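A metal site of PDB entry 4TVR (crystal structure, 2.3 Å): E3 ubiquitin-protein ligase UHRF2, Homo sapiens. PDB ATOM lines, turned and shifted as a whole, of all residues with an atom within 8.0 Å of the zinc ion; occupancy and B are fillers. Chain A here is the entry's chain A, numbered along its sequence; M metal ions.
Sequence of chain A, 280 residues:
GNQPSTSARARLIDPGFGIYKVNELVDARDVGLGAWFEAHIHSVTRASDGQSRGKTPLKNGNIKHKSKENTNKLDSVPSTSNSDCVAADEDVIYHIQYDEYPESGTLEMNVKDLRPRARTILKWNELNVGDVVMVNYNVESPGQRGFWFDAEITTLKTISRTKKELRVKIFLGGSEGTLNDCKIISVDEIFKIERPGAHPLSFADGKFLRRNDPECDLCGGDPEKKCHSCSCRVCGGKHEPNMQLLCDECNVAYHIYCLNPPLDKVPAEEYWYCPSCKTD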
ATOM      1  N   CYS A 216      -4.939 -21.380 -17.450  1.00  0.00           N
ATOM      2  CA  CYS A 216      -4.280 -20.220 -16.852  1.00  0.00           C
ATOM      3  C   CYS A 216      -5.149 -19.567 -15.770  1.00  0.00           C
ATOM      4  O   CYS A 216      -6.289 -19.175 -16.040  1.00  0.00           O
ATOM      5  CB  CYS A 216      -3.937 -19.192 -17.933  1.00  0.00           C
ATOM      6  SG  CYS A 216      -3.198 -17.658 -17.299  1.00  0.00           S
ATOM      7  N   ASP A 217      -4.599 -19.442 -14.572  1.00  0.00           N
ATOM      8  CA  ASP A 217      -5.288 -18.798 -13.444  1.00  0.00           C
ATOM      9  C   ASP A 217      -5.418 -17.280 -13.601  1.00  0.00           C
ATOM     10  O   ASP A 217      -6.358 -16.686 -13.060  1.00  0.00           O
ATOM     11  CB  ASP A 217      -4.551 -19.090 -12.137  1.00  0.00           C
ATOM     12  CG  ASP A 217      -4.665 -20.535 -11.702  1.00  0.00           C
ATOM     13  OD1 ASP A 217      -5.043 -21.391 -12.537  1.00  0.00           O
ATOM     14  OD2 ASP A 217      -4.384 -20.819 -10.517  1.00  0.00           O
ATOM     15  N   LEU A 218      -4.477 -16.665 -14.302  1.00  0.00           N
ATOM     16  CA  LEU A 218      -4.422 -15.210 -14.408  1.00  0.00           C
ATOM     17  C   LEU A 218      -5.519 -14.659 -15.321  1.00  0.00           C
ATOM     18  O   LEU A 218      -6.529 -14.126 -14.843  1.00  0.00           O
ATOM     19  CB  LEU A 218      -3.041 -14.760 -14.907  1.00  0.00           C
ATOM     20  N   CYS A 219      -5.334 -14.789 -16.632  1.00  0.00           N
ATOM     21  CA  CYS A 219      -6.263 -14.209 -17.606  1.00  0.00           C
ATOM     22  C   CYS A 219      -7.497 -15.097 -17.846  1.00  0.00           C
ATOM     23  O   CYS A 219      -8.480 -14.628 -18.414  1.00  0.00           O
ATOM     24  CB  CYS A 219      -5.533 -13.902 -18.924  1.00  0.00           C
ATOM     25  SG  CYS A 219      -4.993 -15.341 -19.889  1.00  0.00           S
ATOM     26  N   GLY A 220      -7.429 -16.349 -17.409  1.00  0.00           N
ATOM     27  CA  GLY A 220      -8.552 -17.282 -17.569  1.00  0.00           C
ATOM     28  C   GLY A 220      -8.712 -17.801 -18.989  1.00  0.00           C
ATOM     29  O   GLY A 220      -9.802 -18.233 -19.375  1.00  0.00           O
ATOM     30  N   GLY A 221      -7.626 -17.777 -19.757  1.00  0.00           N
ATOM     31  CA  GLY A 221      -7.655 -18.171 -21.166  1.00  0.00           C
ATOM     32  C   GLY A 221      -8.418 -17.231 -22.100  1.00  0.00           C
ATOM     33  O   GLY A 221      -8.717 -17.609 -23.237  1.00  0.00           O
ATOM     34  N   ASP A 222      -8.708 -16.016 -21.645  1.00  0.00           N
ATOM     35  CA  ASP A 222      -9.474 -15.056 -22.429  1.00  0.00           C
ATOM     36  C   ASP A 222      -8.546 -14.317 -23.405  1.00  0.00           C
ATOM     37  O   ASP A 222      -7.523 -13.781 -22.987  1.00  0.00           O
ATOM     38  CB  ASP A 222     -10.171 -14.038 -21.522  1.00  0.00           C
ATOM     39  N   LYS A 225      -8.063 -10.143 -22.477  1.00  0.00           N
ATOM     40  CA  LYS A 225      -7.218  -9.655 -21.398  1.00  0.00           C
ATOM     41  C   LYS A 225      -5.728  -9.868 -21.670  1.00  0.00           C
ATOM     42  O   LYS A 225      -5.331 -10.924 -22.178  1.00  0.00           O
ATOM     43  CB  LYS A 225      -7.596 -10.327 -20.075  1.00  0.00           C
ATOM     44  N   LYS A 226      -4.915  -8.878 -21.329  1.00  0.00           N
ATOM     45  CA  LYS A 226      -3.456  -9.001 -21.425  1.00  0.00           C
ATOM     46  C   LYS A 226      -2.966 -10.038 -20.435  1.00  0.00           C
ATOM     47  O   LYS A 226      -3.622 -10.296 -19.411  1.00  0.00           O
ATOM     48  CB  LYS A 226      -2.791  -7.650 -21.149  1.00  0.00           C
ATOM     49  N   CYS A 227      -1.819 -10.658 -20.724  1.00  0.00           N
ATOM     50  CA  CYS A 227      -1.252 -11.682 -19.843  1.00  0.00           C
ATOM     51  C   CYS A 227       0.268 -11.773 -19.950  1.00  0.00           C
ATOM     52  O   CYS A 227       0.802 -12.162 -20.986  1.00  0.00           O
ATOM     53  CB  CYS A 227      -1.877 -13.047 -20.123  1.00  0.00           C
ATOM     54  SG  CYS A 227      -1.947 -14.111 -18.666  1.00  0.00           S
ATOM     55  N   HIS A 228       0.958 -11.420 -18.868  1.00  0.00           N
ATOM     56  CA  HIS A 228       2.408 -11.596 -18.768  1.00  0.00           C
ATOM     57  C   HIS A 228       2.812 -13.066 -18.562  1.00  0.00           C
ATOM     58  O   HIS A 228       3.985 -13.422 -18.760  1.00  0.00           O
ATOM     59  CB  HIS A 228       2.973 -10.753 -17.608  1.00  0.00           C
ATOM     60  CG  HIS A 228       3.026  -9.282 -17.900  1.00  0.00           C
ATOM     61  ND1 HIS A 228       4.196  -8.632 -18.213  1.00  0.00           N
ATOM     62  CD2 HIS A 228       2.058  -8.339 -17.894  1.00  0.00           C
ATOM     63  CE1 HIS A 228       3.950  -7.347 -18.410  1.00  0.00           C
ATOM     64  NE2 HIS A 228       2.653  -7.139 -18.218  1.00  0.00           N
ATOM     65  N   SER A 229       1.862 -13.904 -18.176  1.00  0.00           N
ATOM     66  CA  SER A 229       2.127 -15.294 -17.789  1.00  0.00           C
ATOM     67  C   SER A 229       2.109 -16.260 -18.985  1.00  0.00           C
ATOM     68  O   SER A 229       3.028 -17.060 -19.155  1.00  0.00           O
ATOM     69  CB  SER A 229       1.119 -15.749 -16.732  1.00  0.00           C
ATOM     70  OG  SER A 229       1.543 -16.940 -16.108  1.00  0.00           O
ATOM     71  N   CYS A 230       1.054 -16.179 -19.792  1.00  0.00           N
ATOM     72  CA  CYS A 230       0.873 -17.082 -20.940  1.00  0.00           C
ATOM     73  C   CYS A 230       1.159 -16.412 -22.292  1.00  0.00           C
ATOM     74  O   CYS A 230       0.938 -17.029 -23.344  1.00  0.00           O
ATOM     75  CB  CYS A 230      -0.544 -17.655 -20.936  1.00  0.00           C
ATOM     76  SG  CYS A 230      -1.847 -16.429 -21.139  1.00  0.00           S
ATOM     77  N   SER A 231       1.647 -15.173 -22.271  1.00  0.00           N
ATOM     78  CA  SER A 231       2.039 -14.441 -23.477  1.00  0.00           C
ATOM     79  C   SER A 231       3.361 -13.697 -23.233  1.00  0.00           C
ATOM     80  O   SER A 231       4.142 -14.109 -22.361  1.00  0.00           O
ATOM     81  CB  SER A 231       0.926 -13.487 -23.912  1.00  0.00           C
ATOM     82  OG  SER A 231       1.189 -12.929 -25.184  1.00  0.00           O
ATOM     83  N   LYS A 238      -0.817 -10.433 -26.631  1.00  0.00           N
ATOM     84  CA  LYS A 238      -1.036 -11.627 -27.459  1.00  0.00           C
ATOM     85  C   LYS A 238      -1.051 -11.292 -28.953  1.00  0.00           C
ATOM     86  O   LYS A 238      -1.046 -12.210 -29.789  1.00  0.00           O
ATOM     87  CB  LYS A 238      -2.334 -12.322 -27.058  1.00  0.00           C
ATOM     88  CG  LYS A 238      -2.261 -12.993 -25.703  1.00  0.00           C
ATOM     89  CD  LYS A 238      -3.642 -13.296 -25.142  1.00  0.00           C
ATOM     90  CE  LYS A 238      -3.545 -13.839 -23.725  1.00  0.00           C
ATOM     91  NZ  LYS A 238      -4.870 -13.867 -23.043  1.00  0.00           N
HETATM   92 ZN    ZN M   1      -2.956 -16.185 -19.087  1.00  0.00          ZN
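SG of Cys 216 lies close to N of Leu 218, at 3.4 Å. SG of Cys 219 lies close to NZ of Lys 238, 3.5 Å away. The side-chain sulfur (SG) of Cys 219 sits close to the backbone NH (N) of Gly 221, 3.6 Å away.
Of the 15 residues printed, 4 come within 4 Å of the zinc ion.
The zinc ion is bound by the side-chain sulfur (SG) of Cys 216 (2.3 Å), the side-chain sulfur (SG) of Cys 227 (2.3 Å), the side-chain sulfur (SG) of Cys 230 (2.3 Å) and the side-chain sulfur (SG) of Cys 219 (2.3 Å). The zinc ion has four donor atoms within binding distance.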
